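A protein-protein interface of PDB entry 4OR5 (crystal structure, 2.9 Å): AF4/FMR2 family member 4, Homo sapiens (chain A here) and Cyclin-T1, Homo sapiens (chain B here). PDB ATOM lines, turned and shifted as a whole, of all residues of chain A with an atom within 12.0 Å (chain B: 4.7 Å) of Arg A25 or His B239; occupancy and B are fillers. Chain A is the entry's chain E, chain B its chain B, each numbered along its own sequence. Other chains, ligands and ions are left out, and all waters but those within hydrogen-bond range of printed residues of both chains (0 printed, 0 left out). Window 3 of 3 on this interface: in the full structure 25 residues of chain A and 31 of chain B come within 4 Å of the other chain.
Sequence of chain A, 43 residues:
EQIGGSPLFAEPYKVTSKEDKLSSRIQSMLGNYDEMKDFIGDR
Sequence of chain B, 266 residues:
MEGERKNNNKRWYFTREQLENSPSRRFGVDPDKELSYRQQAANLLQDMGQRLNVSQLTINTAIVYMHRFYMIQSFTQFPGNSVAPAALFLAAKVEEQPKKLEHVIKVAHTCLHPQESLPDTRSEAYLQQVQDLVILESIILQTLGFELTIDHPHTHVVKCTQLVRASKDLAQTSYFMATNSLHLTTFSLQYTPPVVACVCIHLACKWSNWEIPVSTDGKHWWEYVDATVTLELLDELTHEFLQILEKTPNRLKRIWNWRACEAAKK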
ATOM      1  N   LYS A  18     -11.125 -36.752  13.904  1.00  0.00           N
ATOM      2  CA  LYS A  18     -11.425 -35.520  13.181  1.00  0.00           C
ATOM      3  C   LYS A  18     -10.981 -35.276  11.742  1.00  0.00           C
ATOM      4  O   LYS A  18     -10.054 -35.888  11.205  1.00  0.00           O
ATOM      5  CB  LYS A  18     -10.966 -34.326  14.024  1.00  0.00           C
ATOM      6  CG  LYS A  18      -9.695 -34.585  14.801  1.00  0.00           C
ATOM      7  CD  LYS A  18      -8.853 -33.338  14.910  1.00  0.00           C
ATOM      8  CE  LYS A  18      -8.524 -32.804  13.522  1.00  0.00           C
ATOM      9  NZ  LYS A  18      -8.045 -33.874  12.594  1.00  0.00           N
ATOM     10  N   GLU A  19     -11.701 -34.326  11.157  1.00  0.00           N
ATOM     11  CA  GLU A  19     -11.538 -33.814   9.804  1.00  0.00           C
ATOM     12  C   GLU A  19     -11.794 -32.329  10.053  1.00  0.00           C
ATOM     13  O   GLU A  19     -12.625 -31.712   9.388  1.00  0.00           O
ATOM     14  CB  GLU A  19     -12.637 -34.361   8.885  1.00  0.00           C
ATOM     15  CG  GLU A  19     -12.325 -35.662   8.155  1.00  0.00           C
ATOM     16  CD  GLU A  19     -11.570 -35.447   6.845  1.00  0.00           C
ATOM     17  OE1 GLU A  19     -11.539 -36.381   6.007  1.00  0.00           O
ATOM     18  OE2 GLU A  19     -11.004 -34.347   6.652  1.00  0.00           O
ATOM     19  N   ASP A  20     -11.084 -31.778  11.038  1.00  0.00           N
ATOM     20  CA  ASP A  20     -11.223 -30.379  11.459  1.00  0.00           C
ATOM     21  C   ASP A  20     -10.044 -29.472  11.072  1.00  0.00           C
ATOM     22  O   ASP A  20      -9.015 -29.457  11.759  1.00  0.00           O
ATOM     23  CB  ASP A  20     -11.399 -30.353  12.979  1.00  0.00           C
ATOM     24  CG  ASP A  20     -11.487 -28.946  13.547  1.00  0.00           C
ATOM     25  OD1 ASP A  20     -10.957 -28.010  12.912  1.00  0.00           O
ATOM     26  OD2 ASP A  20     -12.072 -28.781  14.644  1.00  0.00           O
ATOM     27  N   LYS A  21     -10.218 -28.691  10.002  1.00  0.00           N
ATOM     28  CA  LYS A  21      -9.177 -27.782   9.508  1.00  0.00           C
ATOM     29  C   LYS A  21      -8.654 -26.828  10.583  1.00  0.00           C
ATOM     30  O   LYS A  21      -7.465 -26.518  10.643  1.00  0.00           O
ATOM     31  CB  LYS A  21      -9.706 -26.977   8.308  1.00  0.00           C
ATOM     32  CG  LYS A  21      -9.799 -27.764   6.990  1.00  0.00           C
ATOM     33  CD  LYS A  21     -10.454 -26.936   5.883  1.00  0.00           C
ATOM     34  CE  LYS A  21     -10.356 -27.621   4.522  1.00  0.00           C
ATOM     35  NZ  LYS A  21      -8.943 -27.742   4.042  1.00  0.00           N
ATOM     36  N   LEU A  22      -9.551 -26.361  11.432  1.00  0.00           N
ATOM     37  CA  LEU A  22      -9.159 -25.452  12.485  1.00  0.00           C
ATOM     38  C   LEU A  22      -8.129 -26.124  13.366  1.00  0.00           C
ATOM     39  O   LEU A  22      -7.092 -25.545  13.648  1.00  0.00           O
ATOM     40  CB  LEU A  22     -10.373 -25.063  13.317  1.00  0.00           C
ATOM     41  CG  LEU A  22     -10.545 -23.569  13.581  1.00  0.00           C
ATOM     42  CD1 LEU A  22     -10.726 -22.827  12.255  1.00  0.00           C
ATOM     43  CD2 LEU A  22     -11.741 -23.362  14.500  1.00  0.00           C
ATOM     44  N   SER A  23      -8.408 -27.356  13.788  1.00  0.00           N
ATOM     45  CA  SER A  23      -7.492 -28.112  14.656  1.00  0.00           C
ATOM     46  C   SER A  23      -6.187 -28.462  13.954  1.00  0.00           C
ATOM     47  O   SER A  23      -5.107 -28.288  14.514  1.00  0.00           O
ATOM     48  CB  SER A  23      -8.165 -29.392  15.153  1.00  0.00           C
ATOM     49  OG  SER A  23      -9.333 -29.078  15.895  1.00  0.00           O
ATOM     50  N   SER A  24      -6.296 -28.962  12.730  1.00  0.00           N
ATOM     51  CA  SER A  24      -5.119 -29.306  11.953  1.00  0.00           C
ATOM     52  C   SER A  24      -4.193 -28.104  11.895  1.00  0.00           C
ATOM     53  O   SER A  24      -2.986 -28.229  12.122  1.00  0.00           O
ATOM     54  CB  SER A  24      -5.519 -29.668  10.533  1.00  0.00           C
ATOM     55  OG  SER A  24      -6.880 -30.042  10.495  1.00  0.00           O
ATOM     56  N   ARG A  25      -4.777 -26.942  11.591  1.00  0.00           N
ATOM     57  CA  ARG A  25      -4.032 -25.701  11.472  1.00  0.00           C
ATOM     58  C   ARG A  25      -3.297 -25.333  12.739  1.00  0.00           C
ATOM     59  O   ARG A  25      -2.088 -25.106  12.715  1.00  0.00           O
ATOM     60  CB  ARG A  25      -4.963 -24.550  11.066  1.00  0.00           C
ATOM     61  CG  ARG A  25      -5.421 -24.602   9.609  1.00  0.00           C
ATOM     62  CD  ARG A  25      -6.387 -23.476   9.269  1.00  0.00           C
ATOM     63  NE  ARG A  25      -5.829 -22.168   9.600  1.00  0.00           N
ATOM     64  CZ  ARG A  25      -6.521 -21.032   9.570  1.00  0.00           C
ATOM     65  NH1 ARG A  25      -7.800 -21.041   9.219  1.00  0.00           N
ATOM     66  NH2 ARG A  25      -5.937 -19.889   9.910  1.00  0.00           N
ATOM     67  N   ILE A  26      -4.016 -25.280  13.849  1.00  0.00           N
ATOM     68  CA  ILE A  26      -3.395 -24.912  15.112  1.00  0.00           C
ATOM     69  C   ILE A  26      -2.344 -25.954  15.504  1.00  0.00           C
ATOM     70  O   ILE A  26      -1.397 -25.650  16.229  1.00  0.00           O
ATOM     71  CB  ILE A  26      -4.477 -24.761  16.223  1.00  0.00           C
ATOM     72  CG1 ILE A  26      -3.844 -24.429  17.579  1.00  0.00           C
ATOM     73  CG2 ILE A  26      -5.289 -26.044  16.316  1.00  0.00           C
ATOM     74  CD1 ILE A  26      -2.919 -23.257  17.567  1.00  0.00           C
ATOM     75  N   GLN A  27      -2.507 -27.179  15.004  1.00  0.00           N
ATOM     76  CA  GLN A  27      -1.570 -28.252  15.301  1.00  0.00           C
ATOM     77  C   GLN A  27      -0.269 -28.076  14.540  1.00  0.00           C
ATOM     78  O   GLN A  27       0.809 -28.157  15.127  1.00  0.00           O
ATOM     79  CB  GLN A  27      -2.182 -29.614  14.958  1.00  0.00           C
ATOM     80  CG  GLN A  27      -2.960 -30.265  16.102  1.00  0.00           C
ATOM     81  CD  GLN A  27      -3.645 -31.562  15.685  1.00  0.00           C
ATOM     82  OE1 GLN A  27      -3.040 -32.410  15.016  1.00  0.00           O
ATOM     83  NE2 GLN A  27      -4.912 -31.726  16.088  1.00  0.00           N
ATOM     84  N   SER A  28      -0.368 -27.825  13.240  1.00  0.00           N
ATOM     85  CA  SER A  28       0.808 -27.662  12.394  1.00  0.00           C
ATOM     86  C   SER A  28       1.651 -26.479  12.803  1.00  0.00           C
ATOM     87  O   SER A  28       2.806 -26.355  12.417  1.00  0.00           O
ATOM     88  CB  SER A  28       0.360 -27.462  10.973  1.00  0.00           C
ATOM     89  OG  SER A  28      -0.850 -28.157  10.780  1.00  0.00           O
ATOM     90  N   MET A  29       1.061 -25.600  13.588  1.00  0.00           N
ATOM     91  CA  MET A  29       1.751 -24.411  14.037  1.00  0.00           C
ATOM     92  C   MET A  29       2.560 -24.651  15.298  1.00  0.00           C
ATOM     93  O   MET A  29       3.748 -24.366  15.342  1.00  0.00           O
ATOM     94  CB  MET A  29       0.726 -23.302  14.297  1.00  0.00           C
ATOM     95  CG  MET A  29       0.209 -22.605  13.057  1.00  0.00           C
ATOM     96  SD  MET A  29       1.498 -21.533  12.524  1.00  0.00           S
ATOM     97  CE  MET A  29       1.674 -20.554  14.032  1.00  0.00           C
ATOM     98  N   LEU A  30       1.903 -25.184  16.321  1.00  0.00           N
ATOM     99  CA  LEU A  30       2.530 -25.434  17.615  1.00  0.00           C
ATOM    100  C   LEU A  30       3.053 -26.858  17.851  1.00  0.00           C
ATOM    101  O   LEU A  30       3.918 -27.072  18.702  1.00  0.00           O
ATOM    102  CB  LEU A  30       1.537 -25.066  18.715  1.00  0.00           C
ATOM    103  CG  LEU A  30       1.044 -23.621  18.621  1.00  0.00           C
ATOM    104  CD1 LEU A  30      -0.260 -23.451  19.382  1.00  0.00           C
ATOM    105  CD2 LEU A  30       2.114 -22.697  19.164  1.00  0.00           C
ATOM    106  N   GLY A  31       2.523 -27.821  17.104  1.00  0.00           N
ATOM    107  CA  GLY A  31       2.957 -29.196  17.257  1.00  0.00           C
ATOM    108  C   GLY A  31       1.906 -30.011  17.970  1.00  0.00           C
ATOM    109  O   GLY A  31       0.820 -29.498  18.240  1.00  0.00           O
ATOM    110  N   ASN A  32       2.217 -31.270  18.274  1.00  0.00           N
ATOM    111  CA  ASN A  32       1.275 -32.140  18.968  1.00  0.00           C
ATOM    112  C   ASN A  32       1.123 -31.642  20.398  1.00  0.00           C
ATOM    113  O   ASN A  32       2.121 -31.436  21.099  1.00  0.00           O
ATOM    114  CB  ASN A  32       1.787 -33.578  18.965  1.00  0.00           C
ATOM    115  CG  ASN A  32       0.782 -34.554  19.541  1.00  0.00           C
ATOM    116  OD1 ASN A  32       0.492 -34.539  20.740  1.00  0.00           O
ATOM    117  ND2 ASN A  32       0.238 -35.407  18.684  1.00  0.00           N
ATOM    118  N   TYR A  33      -0.122 -31.446  20.827  1.00  0.00           N
ATOM    119  CA  TYR A  33      -0.393 -30.929  22.168  1.00  0.00           C
ATOM    120  C   TYR A  33       0.130 -31.804  23.318  1.00  0.00           C
ATOM    121  O   TYR A  33       0.796 -31.304  24.231  1.00  0.00           O
ATOM    122  CB  TYR A  33      -1.904 -30.664  22.341  1.00  0.00           C
ATOM    123  CG  TYR A  33      -2.296 -30.284  23.756  1.00  0.00           C
ATOM    124  CD1 TYR A  33      -1.807 -29.124  24.354  1.00  0.00           C
ATOM    125  CD2 TYR A  33      -3.125 -31.105  24.511  1.00  0.00           C
ATOM    126  CE1 TYR A  33      -2.133 -28.793  25.675  1.00  0.00           C
ATOM    127  CE2 TYR A  33      -3.463 -30.782  25.827  1.00  0.00           C
ATOM    128  CZ  TYR A  33      -2.969 -29.625  26.408  1.00  0.00           C
ATOM    129  OH  TYR A  33      -3.339 -29.293  27.710  1.00  0.00           O
ATOM    130  N   MET A  36       4.083 -31.286  23.650  1.00  0.00           N
ATOM    131  CA  MET A  36       4.500 -29.960  24.117  1.00  0.00           C
ATOM    132  C   MET A  36       3.941 -29.605  25.488  1.00  0.00           C
ATOM    133  O   MET A  36       4.668 -29.160  26.385  1.00  0.00           O
ATOM    134  CB  MET A  36       4.037 -28.915  23.114  1.00  0.00           C
ATOM    135  CG  MET A  36       4.354 -29.267  21.678  1.00  0.00           C
ATOM    136  SD  MET A  36       6.125 -29.455  21.392  1.00  0.00           S
ATOM    137  CE  MET A  36       6.088 -30.387  19.752  1.00  0.00           C
ATOM    138  N   ASP B 235     -15.590 -19.832  15.660  1.00  0.00           N
ATOM    139  CA  ASP B 235     -14.824 -20.370  14.553  1.00  0.00           C
ATOM    140  C   ASP B 235     -14.229 -19.255  13.704  1.00  0.00           C
ATOM    141  O   ASP B 235     -13.099 -19.378  13.220  1.00  0.00           O
ATOM    142  CB  ASP B 235     -15.708 -21.272  13.698  1.00  0.00           C
ATOM    143  CG  ASP B 235     -16.259 -22.450  14.481  1.00  0.00           C
ATOM    144  OD1 ASP B 235     -15.448 -23.251  15.009  1.00  0.00           O
ATOM    145  OD2 ASP B 235     -17.503 -22.575  14.574  1.00  0.00           O
ATOM    146  N   GLU B 236     -14.981 -18.170  13.526  1.00  0.00           N
ATOM    147  CA  GLU B 236     -14.488 -17.056  12.731  1.00  0.00           C
ATOM    148  C   GLU B 236     -13.273 -16.412  13.390  1.00  0.00           C
ATOM    149  O   GLU B 236     -12.234 -16.236  12.763  1.00  0.00           O
ATOM    150  CB  GLU B 236     -15.583 -16.002  12.534  1.00  0.00           C
ATOM    151  CG  GLU B 236     -15.091 -14.755  11.790  1.00  0.00           C
ATOM    152  CD  GLU B 236     -16.148 -13.661  11.616  1.00  0.00           C
ATOM    153  OE1 GLU B 236     -16.696 -13.174  12.635  1.00  0.00           O
ATOM    154  OE2 GLU B 236     -16.416 -13.279  10.452  1.00  0.00           O
ATOM    155  N   LEU B 237     -13.400 -16.072  14.663  1.00  0.00           N
ATOM    156  CA  LEU B 237     -12.305 -15.431  15.366  1.00  0.00           C
ATOM    157  C   LEU B 237     -11.115 -16.356  15.546  1.00  0.00           C
ATOM    158  O   LEU B 237      -9.969 -15.904  15.534  1.00  0.00           O
ATOM    159  CB  LEU B 237     -12.780 -14.894  16.724  1.00  0.00           C
ATOM    160  CG  LEU B 237     -13.896 -13.838  16.671  1.00  0.00           C
ATOM    161  CD1 LEU B 237     -13.946 -13.052  17.961  1.00  0.00           C
ATOM    162  CD2 LEU B 237     -13.628 -12.905  15.524  1.00  0.00           C
ATOM    163  N   THR B 238     -11.385 -17.645  15.717  1.00  0.00           N
ATOM    164  CA  THR B 238     -10.314 -18.620  15.883  1.00  0.00           C
ATOM    165  C   THR B 238      -9.544 -18.669  14.576  1.00  0.00           C
ATOM    166  O   THR B 238      -8.322 -18.864  14.555  1.00  0.00           O
ATOM    167  CB  THR B 238     -10.878 -20.015  16.207  1.00  0.00           C
ATOM    168  OG1 THR B 238     -11.321 -20.021  17.564  1.00  0.00           O
ATOM    169  CG2 THR B 238      -9.822 -21.100  16.022  1.00  0.00           C
ATOM    170  N   HIS B 239     -10.277 -18.476  13.486  1.00  0.00           N
ATOM    171  CA  HIS B 239      -9.674 -18.479  12.168  1.00  0.00           C
ATOM    172  C   HIS B 239      -8.730 -17.302  12.046  1.00  0.00           C
ATOM    173  O   HIS B 239      -7.602 -17.444  11.604  1.00  0.00           O
ATOM    174  CB  HIS B 239     -10.736 -18.354  11.081  1.00  0.00           C
ATOM    175  CG  HIS B 239     -10.176 -17.975   9.747  1.00  0.00           C
ATOM    176  ND1 HIS B 239      -9.472 -18.857   8.954  1.00  0.00           N
ATOM    177  CD2 HIS B 239     -10.195 -16.800   9.073  1.00  0.00           C
ATOM    178  CE1 HIS B 239      -9.086 -18.243   7.850  1.00  0.00           C
ATOM    179  NE2 HIS B 239      -9.512 -16.993   7.898  1.00  0.00           N
ATOM    180  N   GLU B 240      -9.197 -16.127  12.437  1.00  0.00           N
ATOM    181  CA  GLU B 240      -8.361 -14.949  12.319  1.00  0.00           C
ATOM    182  C   GLU B 240      -7.112 -15.081  13.165  1.00  0.00           C
ATOM    183  O   GLU B 240      -6.016 -14.733  12.717  1.00  0.00           O
ATOM    184  CB  GLU B 240      -9.142 -13.690  12.701  1.00  0.00           C
ATOM    185  CG  GLU B 240     -10.277 -13.320  11.738  1.00  0.00           C
ATOM    186  CD  GLU B 240      -9.828 -13.160  10.281  1.00  0.00           C
ATOM    187  OE1 GLU B 240      -8.805 -12.470  10.028  1.00  0.00           O
ATOM    188  OE2 GLU B 240     -10.516 -13.722   9.389  1.00  0.00           O
ATOM    189  N   PHE B 241      -7.277 -15.587  14.383  1.00  0.00           N
ATOM    190  CA  PHE B 241      -6.144 -15.781  15.289  1.00  0.00           C
ATOM    191  C   PHE B 241      -5.133 -16.723  14.623  1.00  0.00           C
ATOM    192  O   PHE B 241      -3.927 -16.518  14.713  1.00  0.00           O
ATOM    193  CB  PHE B 241      -6.643 -16.363  16.612  1.00  0.00           C
ATOM    194  CG  PHE B 241      -5.646 -16.297  17.735  1.00  0.00           C
ATOM    195  CD1 PHE B 241      -6.017 -15.776  18.966  1.00  0.00           C
ATOM    196  CD2 PHE B 241      -4.366 -16.812  17.587  1.00  0.00           C
ATOM    197  CE1 PHE B 241      -5.119 -15.769  20.044  1.00  0.00           C
ATOM    198  CE2 PHE B 241      -3.464 -16.818  18.651  1.00  0.00           C
ATOM    199  CZ  PHE B 241      -3.840 -16.292  19.888  1.00  0.00           C
ATOM    200  N   LEU B 242      -5.614 -17.752  13.938  1.00  0.00           N
ATOM    201  CA  LEU B 242      -4.688 -18.655  13.262  1.00  0.00           C
ATOM    202  C   LEU B 242      -3.979 -17.900  12.148  1.00  0.00           C
ATOM    203  O   LEU B 242      -2.768 -18.001  12.013  1.00  0.00           O
ATOM    204  CB  LEU B 242      -5.425 -19.874  12.704  1.00  0.00           C
ATOM    205  CG  LEU B 242      -5.860 -20.890  13.764  1.00  0.00           C
ATOM    206  CD1 LEU B 242      -6.777 -21.934  13.146  1.00  0.00           C
ATOM    207  CD2 LEU B 242      -4.619 -21.529  14.378  1.00  0.00           C
ATOM    208  N   GLN B 243      -4.741 -17.139  11.363  1.00  0.00           N
ATOM    209  CA  GLN B 243      -4.190 -16.311  10.283  1.00  0.00           C
ATOM    210  C   GLN B 243      -3.007 -15.483  10.820  1.00  0.00           C
ATOM    211  O   GLN B 243      -1.945 -15.440  10.207  1.00  0.00           O
ATOM    212  CB  GLN B 243      -5.262 -15.341   9.729  1.00  0.00           C
ATOM    213  CG  GLN B 243      -6.390 -16.003   8.925  1.00  0.00           C
ATOM    214  CD  GLN B 243      -6.993 -15.104   7.829  1.00  0.00           C
ATOM    215  OE1 GLN B 243      -7.662 -14.107   8.111  1.00  0.00           O
ATOM    216  NE2 GLN B 243      -6.748 -15.468   6.572  1.00  0.00           N
ATOM    217  N   GLU B 246      -0.080 -17.708  11.683  1.00  0.00           N
ATOM    218  CA  GLU B 246       0.566 -18.205  10.491  1.00  0.00           C
ATOM    219  C   GLU B 246       1.365 -17.137   9.746  1.00  0.00           C
ATOM    220  O   GLU B 246       2.134 -17.467   8.851  1.00  0.00           O
ATOM    221  CB  GLU B 246      -0.490 -18.828   9.582  1.00  0.00           C
ATOM    222  CG  GLU B 246      -1.358 -19.828  10.323  1.00  0.00           C
ATOM    223  CD  GLU B 246      -2.560 -20.287   9.525  1.00  0.00           C
ATOM    224  OE1 GLU B 246      -3.290 -21.195   9.996  1.00  0.00           O
ATOM    225  OE2 GLU B 246      -2.774 -19.740   8.429  1.00  0.00           O
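Among the printed residues, merely in contact across the chains: Leu A22 with Asp B235 (3.7 Å), Leu A22 with Thr B238 (3.3 Å), Leu A22 with Leu B242 (3.7 Å), Arg A25 with Leu B242 (2.8 Å), Ile A26 with Leu B242 (3.7 Å) and Met A29 with Glu B246 (3.99 Å).
OE1 of Glu B246 lies within salt-bridge range of NE of Arg A25, at 2.7 Å. The guanidinium group (NH2) of Arg A25 sits close to the backbone NH (N) of Gln B243 (3.3 Å). A ring nitrogen (ND1) of His B239 is in hydrogen-bond range of the guanidinium group (NH1) of Arg A25 (2.8 Å).
Of the 17 printed residues of chain A, 4 touch a printed residue of chain B. Hydrophobic or aromatic side chains of chain A that line the printed part of chain B: Leu A22, Ile A26 and Met A29. Of the 10 printed residues of chain B, 6 touch a printed residue of chain A. Along chain B the printed residues that touch a printed residue of chain A span positions 235 to 246.
A ring nitrogen (NE2) of His B239 lies close to the side-chain amide nitrogen of Gln B243 (3.4 Å). The backbone NH (N) of Leu A22 is in hydrogen-bond range of the side-chain carboxylate (OD1) of Asp A20 (2.6 Å).
Of chain B, only His B239, Leu B242, Gln B243 and Glu B246 come within 4 Å of Arg A25. Of chain A, only Arg A25 (2.8 Å) comes within 4 Å of His B239. No residue of chain A comes within 4 Å of Leu B237. Of chain A, only Leu A22 comes within 4 Å of Thr B238. No residue of chain A comes within 4 Å of Glu B240. Leu B242 touches three residues of chain A. Printed residues of chain B within 4 Å of Ile A26: Leu B242 (3.7 Å). Of the printed residues of chain B, Leu A22 touches Asp B235, Thr B238 and Leu B242. Of the printed residues of chain A, Asp B235 touches Leu A22 (3.7 Å). Lys A18 touches none of the printed residues of chain B. Glu A19 touches none of the printed residues of chain B. The nearest printed residue of chain B that does not touch Arg A25 is Thr B238 (5.3 Å). The nearest residue of chain A that does not touch His B239 is Leu A22 (4.5 Å).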
